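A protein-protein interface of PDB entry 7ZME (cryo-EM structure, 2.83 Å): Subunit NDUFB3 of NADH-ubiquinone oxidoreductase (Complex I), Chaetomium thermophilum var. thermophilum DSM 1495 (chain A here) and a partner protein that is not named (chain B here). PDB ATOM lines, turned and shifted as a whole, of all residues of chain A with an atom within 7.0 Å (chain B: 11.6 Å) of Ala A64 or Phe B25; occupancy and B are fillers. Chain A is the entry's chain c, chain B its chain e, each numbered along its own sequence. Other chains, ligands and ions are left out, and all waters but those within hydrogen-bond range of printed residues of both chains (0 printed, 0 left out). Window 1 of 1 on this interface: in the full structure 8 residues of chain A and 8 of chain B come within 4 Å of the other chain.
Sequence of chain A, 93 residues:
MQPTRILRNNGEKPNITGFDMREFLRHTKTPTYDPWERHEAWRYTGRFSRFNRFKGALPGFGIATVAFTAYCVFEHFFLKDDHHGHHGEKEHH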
ATOM      1  N   GLY A  60      20.880  -8.770 -15.803  1.00  0.00           N
ATOM      2  CA  GLY A  60      21.870  -7.756 -16.091  1.00  0.00           C
ATOM      3  C   GLY A  60      23.215  -8.260 -16.556  1.00  0.00           C
ATOM      4  O   GLY A  60      24.153  -7.464 -16.663  1.00  0.00           O
ATOM      5  N   PHE A  61      23.342  -9.558 -16.837  1.00  0.00           N
ATOM      6  CA  PHE A  61      24.650 -10.128 -17.142  1.00  0.00           C
ATOM      7  C   PHE A  61      25.221  -9.546 -18.430  1.00  0.00           C
ATOM      8  O   PHE A  61      26.426  -9.278 -18.517  1.00  0.00           O
ATOM      9  CB  PHE A  61      24.537 -11.652 -17.222  1.00  0.00           C
ATOM     10  CG  PHE A  61      25.859 -12.372 -17.181  1.00  0.00           C
ATOM     11  CD1 PHE A  61      26.746 -12.306 -18.243  1.00  0.00           C
ATOM     12  CD2 PHE A  61      26.211 -13.117 -16.070  1.00  0.00           C
ATOM     13  CE1 PHE A  61      27.956 -12.968 -18.197  1.00  0.00           C
ATOM     14  CE2 PHE A  61      27.418 -13.782 -16.018  1.00  0.00           C
ATOM     15  CZ  PHE A  61      28.292 -13.708 -17.083  1.00  0.00           C
ATOM     16  N   GLY A  62      24.375  -9.340 -19.440  1.00  0.00           N
ATOM     17  CA  GLY A  62      24.872  -8.876 -20.725  1.00  0.00           C
ATOM     18  C   GLY A  62      25.499  -7.496 -20.655  1.00  0.00           C
ATOM     19  O   GLY A  62      26.587  -7.267 -21.189  1.00  0.00           O
ATOM     20  N   ILE A  63      24.821  -6.557 -19.993  1.00  0.00           N
ATOM     21  CA  ILE A  63      25.320  -5.184 -19.940  1.00  0.00           C
ATOM     22  C   ILE A  63      26.580  -5.099 -19.091  1.00  0.00           C
ATOM     23  O   ILE A  63      27.526  -4.376 -19.431  1.00  0.00           O
ATOM     24  CB  ILE A  63      24.221  -4.236 -19.428  1.00  0.00           C
ATOM     25  CG1 ILE A  63      23.038  -4.224 -20.397  1.00  0.00           C
ATOM     26  CG2 ILE A  63      24.766  -2.831 -19.242  1.00  0.00           C
ATOM     27  CD1 ILE A  63      21.813  -3.527 -19.856  1.00  0.00           C
ATOM     28  N   ALA A  64      26.621  -5.834 -17.978  1.00  0.00           N
ATOM     29  CA  ALA A  64      27.768  -5.757 -17.079  1.00  0.00           C
ATOM     30  C   ALA A  64      29.044  -6.230 -17.763  1.00  0.00           C
ATOM     31  O   ALA A  64      30.127  -5.685 -17.518  1.00  0.00           O
ATOM     32  CB  ALA A  64      27.503  -6.575 -15.816  1.00  0.00           C
ATOM     33  N   THR A  65      28.938  -7.249 -18.621  1.00  0.00           N
ATOM     34  CA  THR A  65      30.122  -7.768 -19.300  1.00  0.00           C
ATOM     35  C   THR A  65      30.773  -6.701 -20.170  1.00  0.00           C
ATOM     36  O   THR A  65      32.003  -6.570 -20.189  1.00  0.00           O
ATOM     37  CB  THR A  65      29.752  -8.990 -20.140  1.00  0.00           C
ATOM     38  OG1 THR A  65      28.892  -9.850 -19.381  1.00  0.00           O
ATOM     39  CG2 THR A  65      31.002  -9.756 -20.540  1.00  0.00           C
ATOM     40  N   VAL A  66      29.967  -5.931 -20.903  1.00  0.00           N
ATOM     41  CA  VAL A  66      30.512  -4.838 -21.699  1.00  0.00           C
ATOM     42  C   VAL A  66      31.123  -3.773 -20.797  1.00  0.00           C
ATOM     43  O   VAL A  66      32.224  -3.273 -21.060  1.00  0.00           O
ATOM     44  CB  VAL A  66      29.423  -4.249 -22.615  1.00  0.00           C
ATOM     45  CG1 VAL A  66      29.901  -2.954 -23.248  1.00  0.00           C
ATOM     46  CG2 VAL A  66      29.031  -5.257 -23.682  1.00  0.00           C
ATOM     47  N   ALA A  67      30.424  -3.413 -19.719  1.00  0.00           N
ATOM     48  CA  ALA A  67      30.935  -2.392 -18.810  1.00  0.00           C
ATOM     49  C   ALA A  67      32.228  -2.839 -18.141  1.00  0.00           C
ATOM     50  O   ALA A  67      33.163  -2.044 -17.991  1.00  0.00           O
ATOM     51  CB  ALA A  67      29.878  -2.047 -17.760  1.00  0.00           C
ATOM     52  N   PHE A  68      32.298  -4.106 -17.725  1.00  0.00           N
ATOM     53  CA  PHE A  68      33.507  -4.604 -17.080  1.00  0.00           C
ATOM     54  C   PHE A  68      34.695  -4.573 -18.034  1.00  0.00           C
ATOM     55  O   PHE A  68      35.813  -4.231 -17.633  1.00  0.00           O
ATOM     56  CB  PHE A  68      33.282  -6.020 -16.554  1.00  0.00           C
ATOM     57  CG  PHE A  68      34.419  -6.543 -15.725  1.00  0.00           C
ATOM     58  CD1 PHE A  68      34.780  -5.912 -14.547  1.00  0.00           C
ATOM     59  CD2 PHE A  68      35.132  -7.658 -16.130  1.00  0.00           C
ATOM     60  CE1 PHE A  68      35.827  -6.388 -13.784  1.00  0.00           C
ATOM     61  CE2 PHE A  68      36.181  -8.138 -15.370  1.00  0.00           C
ATOM     62  CZ  PHE A  68      36.529  -7.502 -14.197  1.00  0.00           C
ATOM     63  N   THR A  69      34.471  -4.937 -19.298  1.00  0.00           N
ATOM     64  CA  THR A  69      35.548  -4.890 -20.281  1.00  0.00           C
ATOM     65  C   THR A  69      36.039  -3.463 -20.487  1.00  0.00           C
ATOM     66  O   THR A  69      37.245  -3.226 -20.629  1.00  0.00           O
ATOM     67  CB  THR A  69      35.080  -5.495 -21.605  1.00  0.00           C
ATOM     68  OG1 THR A  69      34.677  -6.854 -21.393  1.00  0.00           O
ATOM     69  CG2 THR A  69      36.198  -5.465 -22.635  1.00  0.00           C
ATOM     70  N   ALA A  70      35.117  -2.496 -20.501  1.00  0.00           N
ATOM     71  CA  ALA A  70      35.511  -1.100 -20.654  1.00  0.00           C
ATOM     72  C   ALA A  70      36.376  -0.638 -19.488  1.00  0.00           C
ATOM     73  O   ALA A  70      37.358   0.089 -19.683  1.00  0.00           O
ATOM     74  CB  ALA A  70      34.271  -0.216 -20.786  1.00  0.00           C
ATOM     75  N   TYR A  71      36.025  -1.045 -18.266  1.00  0.00           N
ATOM     76  CA  TYR A  71      36.823  -0.667 -17.104  1.00  0.00           C
ATOM     77  C   TYR A  71      38.215  -1.283 -17.164  1.00  0.00           C
ATOM     78  O   TYR A  71      39.201  -0.636 -16.794  1.00  0.00           O
ATOM     79  CB  TYR A  71      36.111  -1.081 -15.817  1.00  0.00           C
ATOM     80  CG  TYR A  71      37.028  -1.175 -14.619  1.00  0.00           C
ATOM     81  CD1 TYR A  71      37.547  -0.031 -14.029  1.00  0.00           C
ATOM     82  CD2 TYR A  71      37.376  -2.405 -14.081  1.00  0.00           C
ATOM     83  CE1 TYR A  71      38.387  -0.111 -12.934  1.00  0.00           C
ATOM     84  CE2 TYR A  71      38.215  -2.495 -12.987  1.00  0.00           C
ATOM     85  CZ  TYR A  71      38.717  -1.345 -12.417  1.00  0.00           C
ATOM     86  OH  TYR A  71      39.553  -1.429 -11.328  1.00  0.00           O
ATOM     87  N   PHE B  14      13.682  -1.543 -16.043  1.00  0.00           N
ATOM     88  CA  PHE B  14      14.973  -0.905 -15.814  1.00  0.00           C
ATOM     89  C   PHE B  14      15.522  -1.246 -14.435  1.00  0.00           C
ATOM     90  O   PHE B  14      16.724  -1.495 -14.280  1.00  0.00           O
ATOM     91  CB  PHE B  14      14.852   0.608 -15.982  1.00  0.00           C
ATOM     92  CG  PHE B  14      16.082   1.362 -15.567  1.00  0.00           C
ATOM     93  CD1 PHE B  14      17.239   1.294 -16.324  1.00  0.00           C
ATOM     94  CD2 PHE B  14      16.084   2.136 -14.420  1.00  0.00           C
ATOM     95  CE1 PHE B  14      18.374   1.985 -15.946  1.00  0.00           C
ATOM     96  CE2 PHE B  14      17.215   2.830 -14.035  1.00  0.00           C
ATOM     97  CZ  PHE B  14      18.362   2.754 -14.799  1.00  0.00           C
ATOM     98  N   ALA B  16      14.890  -3.945 -12.694  1.00  0.00           N
ATOM     99  CA  ALA B  16      15.306  -5.343 -12.729  1.00  0.00           C
ATOM    100  C   ALA B  16      16.686  -5.491 -13.352  1.00  0.00           C
ATOM    101  O   ALA B  16      17.579  -6.117 -12.772  1.00  0.00           O
ATOM    102  CB  ALA B  16      14.286  -6.168 -13.508  1.00  0.00           C
ATOM    103  N   THR B  17      16.873  -4.918 -14.541  1.00  0.00           N
ATOM    104  CA  THR B  17      18.161  -5.022 -15.216  1.00  0.00           C
ATOM    105  C   THR B  17      19.255  -4.329 -14.416  1.00  0.00           C
ATOM    106  O   THR B  17      20.371  -4.847 -14.299  1.00  0.00           O
ATOM    107  CB  THR B  17      18.062  -4.431 -16.623  1.00  0.00           C
ATOM    108  OG1 THR B  17      17.078  -5.153 -17.374  1.00  0.00           O
ATOM    109  CG2 THR B  17      19.398  -4.532 -17.336  1.00  0.00           C
ATOM    110  N   GLY B  18      18.947  -3.162 -13.847  1.00  0.00           N
ATOM    111  CA  GLY B  18      19.949  -2.437 -13.081  1.00  0.00           C
ATOM    112  C   GLY B  18      20.473  -3.235 -11.904  1.00  0.00           C
ATOM    113  O   GLY B  18      21.681  -3.288 -11.662  1.00  0.00           O
ATOM    114  N   LEU B  19      19.570  -3.868 -11.155  1.00  0.00           N
ATOM    115  CA  LEU B  19      19.997  -4.696 -10.033  1.00  0.00           C
ATOM    116  C   LEU B  19      20.811  -5.889 -10.509  1.00  0.00           C
ATOM    117  O   LEU B  19      21.831  -6.236  -9.905  1.00  0.00           O
ATOM    118  CB  LEU B  19      18.784  -5.155  -9.232  1.00  0.00           C
ATOM    119  CG  LEU B  19      18.041  -4.037  -8.511  1.00  0.00           C
ATOM    120  CD1 LEU B  19      16.801  -4.573  -7.820  1.00  0.00           C
ATOM    121  CD2 LEU B  19      18.964  -3.367  -7.514  1.00  0.00           C
ATOM    122  N   GLY B  20      20.373  -6.533 -11.592  1.00  0.00           N
ATOM    123  CA  GLY B  20      21.148  -7.628 -12.148  1.00  0.00           C
ATOM    124  C   GLY B  20      22.479  -7.164 -12.708  1.00  0.00           C
ATOM    125  O   GLY B  20      23.502  -7.831 -12.531  1.00  0.00           O
ATOM    126  N   ALA B  21      22.482  -6.023 -13.399  1.00  0.00           N
ATOM    127  CA  ALA B  21      23.736  -5.470 -13.897  1.00  0.00           C
ATOM    128  C   ALA B  21      24.641  -5.044 -12.752  1.00  0.00           C
ATOM    129  O   ALA B  21      25.848  -5.304 -12.781  1.00  0.00           O
ATOM    130  CB  ALA B  21      23.461  -4.293 -14.831  1.00  0.00           C
ATOM    131  N   SER B  22      24.078  -4.386 -11.736  1.00  0.00           N
ATOM    132  CA  SER B  22      24.886  -3.980 -10.592  1.00  0.00           C
ATOM    133  C   SER B  22      25.438  -5.191  -9.858  1.00  0.00           C
ATOM    134  O   SER B  22      26.595  -5.185  -9.420  1.00  0.00           O
ATOM    135  CB  SER B  22      24.065  -3.112  -9.638  1.00  0.00           C
ATOM    136  OG  SER B  22      23.016  -3.859  -9.049  1.00  0.00           O
ATOM    137  N   MET B  23      24.626  -6.237  -9.709  1.00  0.00           N
ATOM    138  CA  MET B  23      25.100  -7.450  -9.057  1.00  0.00           C
ATOM    139  C   MET B  23      26.278  -8.040  -9.813  1.00  0.00           C
ATOM    140  O   MET B  23      27.388  -8.130  -9.281  1.00  0.00           O
ATOM    141  CB  MET B  23      23.976  -8.477  -8.941  1.00  0.00           C
ATOM    142  CG  MET B  23      24.455  -9.819  -8.421  1.00  0.00           C
ATOM    143  SD  MET B  23      23.185 -11.091  -8.373  1.00  0.00           S
ATOM    144  CE  MET B  23      22.918 -11.363 -10.118  1.00  0.00           C
ATOM    145  N   TRP B  24      26.061  -8.419 -11.075  1.00  0.00           N
ATOM    146  CA  TRP B  24      27.102  -9.115 -11.823  1.00  0.00           C
ATOM    147  C   TRP B  24      28.357  -8.271 -11.950  1.00  0.00           C
ATOM    148  O   TRP B  24      29.459  -8.759 -11.684  1.00  0.00           O
ATOM    149  CB  TRP B  24      26.588  -9.533 -13.197  1.00  0.00           C
ATOM    150  CG  TRP B  24      25.638 -10.679 -13.123  1.00  0.00           C
ATOM    151  CD1 TRP B  24      24.330 -10.682 -13.495  1.00  0.00           C
ATOM    152  CD2 TRP B  24      25.921 -11.992 -12.629  1.00  0.00           C
ATOM    153  NE1 TRP B  24      23.780 -11.917 -13.270  1.00  0.00           N
ATOM    154  CE2 TRP B  24      24.737 -12.740 -12.738  1.00  0.00           C
ATOM    155  CE3 TRP B  24      27.061 -12.607 -12.109  1.00  0.00           C
ATOM    156  CZ2 TRP B  24      24.659 -14.072 -12.345  1.00  0.00           C
ATOM    157  CZ3 TRP B  24      26.983 -13.927 -11.720  1.00  0.00           C
ATOM    158  CH2 TRP B  24      25.789 -14.647 -11.840  1.00  0.00           C
ATOM    159  N   PHE B  25      28.209  -6.989 -12.296  1.00  0.00           N
ATOM    160  CA  PHE B  25      29.381  -6.126 -12.411  1.00  0.00           C
ATOM    161  C   PHE B  25      30.191  -6.121 -11.126  1.00  0.00           C
ATOM    162  O   PHE B  25      31.410  -5.928 -11.161  1.00  0.00           O
ATOM    163  CB  PHE B  25      28.960  -4.706 -12.775  1.00  0.00           C
ATOM    164  CG  PHE B  25      30.100  -3.729 -12.813  1.00  0.00           C
ATOM    165  CD1 PHE B  25      31.021  -3.760 -13.846  1.00  0.00           C
ATOM    166  CD2 PHE B  25      30.256  -2.788 -11.811  1.00  0.00           C
ATOM    167  CE1 PHE B  25      32.072  -2.866 -13.882  1.00  0.00           C
ATOM    168  CE2 PHE B  25      31.306  -1.892 -11.841  1.00  0.00           C
ATOM    169  CZ  PHE B  25      32.214  -1.931 -12.878  1.00  0.00           C
ATOM    170  N   TRP B  26      29.532  -6.337  -9.986  1.00  0.00           N
ATOM    171  CA  TRP B  26      30.239  -6.417  -8.715  1.00  0.00           C
ATOM    172  C   TRP B  26      31.071  -7.691  -8.614  1.00  0.00           C
ATOM    173  O   TRP B  26      32.206  -7.648  -8.129  1.00  0.00           O
ATOM    174  CB  TRP B  26      29.237  -6.315  -7.566  1.00  0.00           C
ATOM    175  CG  TRP B  26      29.794  -6.620  -6.214  1.00  0.00           C
ATOM    176  CD1 TRP B  26      29.650  -7.780  -5.518  1.00  0.00           C
ATOM    177  CD2 TRP B  26      30.573  -5.751  -5.386  1.00  0.00           C
ATOM    178  NE1 TRP B  26      30.294  -7.693  -4.312  1.00  0.00           N
ATOM    179  CE2 TRP B  26      30.870  -6.456  -4.206  1.00  0.00           C
ATOM    180  CE3 TRP B  26      31.052  -4.447  -5.530  1.00  0.00           C
ATOM    181  CZ2 TRP B  26      31.623  -5.901  -3.176  1.00  0.00           C
ATOM    182  CZ3 TRP B  26      31.798  -3.900  -4.507  1.00  0.00           C
ATOM    183  CH2 TRP B  26      32.076  -4.626  -3.345  1.00  0.00           C
ATOM    184  N   ILE B  27      30.539  -8.834  -9.065  1.00  0.00           N
ATOM    185  CA  ILE B  27      31.291 -10.085  -8.944  1.00  0.00           C
ATOM    186  C   ILE B  27      32.565 -10.044  -9.783  1.00  0.00           C
ATOM    187  O   ILE B  27      33.635 -10.450  -9.319  1.00  0.00           O
ATOM    188  CB  ILE B  27      30.424 -11.313  -9.285  1.00  0.00           C
ATOM    189  CG1 ILE B  27      29.199 -11.412  -8.373  1.00  0.00           C
ATOM    190  CG2 ILE B  27      31.237 -12.590  -9.193  1.00  0.00           C
ATOM    191  CD1 ILE B  27      27.906 -11.047  -9.000  1.00  0.00           C
ATOM    192  N   PHE B  28      32.479  -9.565 -11.028  1.00  0.00           N
ATOM    193  CA  PHE B  28      33.707  -9.406 -11.805  1.00  0.00           C
ATOM    194  C   PHE B  28      34.663  -8.429 -11.134  1.00  0.00           C
ATOM    195  O   PHE B  28      35.870  -8.689 -11.057  1.00  0.00           O
ATOM    196  CB  PHE B  28      33.424  -8.960 -13.244  1.00  0.00           C
ATOM    197  CG  PHE B  28      32.443  -9.825 -13.989  1.00  0.00           C
ATOM    198  CD1 PHE B  28      31.084  -9.702 -13.796  1.00  0.00           C
ATOM    199  CD2 PHE B  28      32.898 -10.761 -14.903  1.00  0.00           C
ATOM    200  CE1 PHE B  28      30.191 -10.496 -14.490  1.00  0.00           C
ATOM    201  CE2 PHE B  28      32.014 -11.560 -15.602  1.00  0.00           C
ATOM    202  CZ  PHE B  28      30.659 -11.427 -15.395  1.00  0.00           C
ATOM    203  N   TYR B  29      34.150  -7.301 -10.643  1.00  0.00           N
ATOM    204  CA  TYR B  29      35.019  -6.336  -9.979  1.00  0.00           C
ATOM    205  C   TYR B  29      35.609  -6.915  -8.699  1.00  0.00           C
ATOM    206  O   TYR B  29      36.797  -6.727  -8.416  1.00  0.00           O
ATOM    207  CB  TYR B  29      34.253  -5.051  -9.681  1.00  0.00           C
ATOM    208  CG  TYR B  29      35.108  -3.981  -9.042  1.00  0.00           C
ATOM    209  CD1 TYR B  29      36.161  -3.403  -9.738  1.00  0.00           C
ATOM    210  CD2 TYR B  29      34.865  -3.552  -7.745  1.00  0.00           C
ATOM    211  CE1 TYR B  29      36.946  -2.427  -9.162  1.00  0.00           C
ATOM    212  CE2 TYR B  29      35.647  -2.576  -7.160  1.00  0.00           C
ATOM    213  CZ  TYR B  29      36.686  -2.018  -7.872  1.00  0.00           C
ATOM    214  OH  TYR B  29      37.467  -1.046  -7.293  1.00  0.00           O
ATOM    215  N   ARG B  30      34.794  -7.621  -7.915  1.00  0.00           N
ATOM    216  CA  ARG B  30      35.281  -8.281  -6.710  1.00  0.00           C
ATOM    217  C   ARG B  30      36.096  -9.530  -7.014  1.00  0.00           C
ATOM    218  O   ARG B  30      36.722 -10.076  -6.100  1.00  0.00           O
ATOM    219  CB  ARG B  30      34.098  -8.619  -5.799  1.00  0.00           C
ATOM    220  CG  ARG B  30      34.434  -8.794  -4.320  1.00  0.00           C
ATOM    221  CD  ARG B  30      35.371  -7.722  -3.802  1.00  0.00           C
ATOM    222  NE  ARG B  30      34.892  -6.373  -4.079  1.00  0.00           N
ATOM    223  CZ  ARG B  30      35.627  -5.282  -3.912  1.00  0.00           C
ATOM    224  NH1 ARG B  30      36.870  -5.384  -3.468  1.00  0.00           N
ATOM    225  NH2 ARG B  30      35.122  -4.088  -4.187  1.00  0.00           N
ATOM    226  N   ALA B  31      36.108  -9.996  -8.265  1.00  0.00           N
ATOM    227  CA  ALA B  31      36.993 -11.080  -8.667  1.00  0.00           C
ATOM    228  C   ALA B  31      38.281 -10.586  -9.301  1.00  0.00           C
ATOM    229  O   ALA B  31      39.276 -11.318  -9.305  1.00  0.00           O
ATOM    230  CB  ALA B  31      36.291 -12.020  -9.650  1.00  0.00           C
ATOM    231  N   LYS B  32      38.282  -9.370  -9.847  1.00  0.00           N
ATOM    232  CA  LYS B  32      39.507  -8.828 -10.421  1.00  0.00           C
ATOM    233  C   LYS B  32      40.541  -8.559  -9.337  1.00  0.00           C
ATOM    234  O   LYS B  32      41.743  -8.748  -9.555  1.00  0.00           O
ATOM    235  CB  LYS B  32      39.195  -7.555 -11.207  1.00  0.00           C
ATOM    236  CG  LYS B  32      40.409  -6.895 -11.838  1.00  0.00           C
ATOM    237  CD  LYS B  32      40.966  -7.747 -12.966  1.00  0.00           C
ATOM    238  CE  LYS B  32      42.060  -7.016 -13.726  1.00  0.00           C
ATOM    239  NZ  LYS B  32      41.507  -5.906 -14.551  1.00  0.00           N
ATOM    240  N   LYS B  33      40.092  -8.124  -8.160  1.00  0.00           N
ATOM    241  CA  LYS B  33      40.986  -7.763  -7.067  1.00  0.00           C
ATOM    242  C   LYS B  33      41.150  -8.896  -6.059  1.00  0.00           C
ATOM    243  O   LYS B  33      42.272  -9.333  -5.788  1.00  0.00           O
ATOM    244  CB  LYS B  33      40.471  -6.496  -6.373  1.00  0.00           C
ATOM    245  CG  LYS B  33      40.561  -5.249  -7.234  1.00  0.00           C
ATOM    246  CD  LYS B  33      40.162  -4.008  -6.455  1.00  0.00           C
ATOM    247  CE  LYS B  33      40.278  -2.760  -7.313  1.00  0.00           C
ATOM    248  NZ  LYS B  33      39.872  -1.536  -6.570  1.00  0.00           N
ATOM    249  N   ASP B  34      40.045  -9.381  -5.494  1.00  0.00           N
ATOM    250  CA  ASP B  34      40.115 -10.409  -4.463  1.00  0.00           C
ATOM    251  C   ASP B  34      40.257 -11.815  -5.024  1.00  0.00           C
ATOM    252  O   ASP B  34      40.546 -12.740  -4.258  1.00  0.00           O
ATOM    253  CB  ASP B  34      38.872 -10.346  -3.570  1.00  0.00           C
ATOM    254  CG  ASP B  34      38.976  -9.278  -2.502  1.00  0.00           C
ATOM    255  OD1 ASP B  34      40.112  -8.909  -2.136  1.00  0.00           O
ATOM    256  OD2 ASP B  34      37.922  -8.808  -2.025  1.00  0.00           O
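Of the 20 printed residues of chain B, 7 touch a printed residue of chain A. Of the 12 printed residues of chain A, 6 touch a printed residue of chain B. Printed residues of chain A that touch a printed residue of chain B: Gly A60, Phe A61, Ile A63, Ala A64, Phe A68 and Tyr A71. Hydrophobic or aromatic side chains of chain A within 4 Å of the printed part of chain B: Phe A61, Ile A63, Ala A64, Phe A68 and Tyr A71. Among the printed residues, 12 pairs touch across the chains. Among the printed residues, no Asp or Glu carboxylate lies within 4 Å of a Lys or Arg side-chain nitrogen of the other chain.
O of Phe A61 is in hydrogen-bond range of OG1 of Thr A65 (2.7 Å). NZ of Lys B33 is in hydrogen-bond range of OH of Tyr B29 (2.6 Å).
Among the printed residues, merely in contact across the chains: Gly A60 with Thr B17 (3.7 Å), Gly A60 with Gly B20 (3.5 Å), Gly A60 with Ala B21 (3.3 Å), Phe A61 with Trp B24 (3.6 Å), Phe A61 with Phe B28 (3.7 Å), Ile A63 with Thr B17 (3.6 Å), Ala A64 with Ala B21 (3.7 Å), Ala A64 with Phe B25 (3.6 Å), Phe A68 with Phe B25 (3.9 Å), Phe A68 with Phe B28 (3.4 Å), Phe A68 with Tyr B29 (3.7 Å) and Tyr A71 with Tyr B29 (3.5 Å).
Ala A64 touches just these residues of chain B: Ala B21 and Phe B25. Phe B25 touches two residues of chain A. Gly A60 touches three residues of chain B. Phe A61 touches just these residues of chain B: Trp B24 and Phe B28. No residue of chain B comes within 4 Å of Gly A62. Of chain B, only Thr B17 comes within 4 Å of Ile A63. No residue of chain B comes within 4 Å of Thr A65. Val A66 touches none of the printed residues of chain B. No residue of chain B comes within 4 Å of Ala A67. Of the printed residues of chain A, Tyr B29 touches Phe A68 (3.7 Å) and Tyr A71 (3.5 Å). Printed residues of chain A within 4 Å of Phe B28: Phe A61 and Phe A68. Of the printed residues of chain A, Trp B24 touches Phe A61. Of the printed residues of chain A, Thr B17 touches Gly A60 and Ile A63. Gly B18 touches none of the printed residues of chain A. Trp B26 touches none of the printed residues of chain A. The nearest residue of chain B that does not touch Ala A64 is Trp B24 (4.1 Å). The nearest residue of chain A that does not touch Phe B25 is Ala A67 (4.3 Å).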
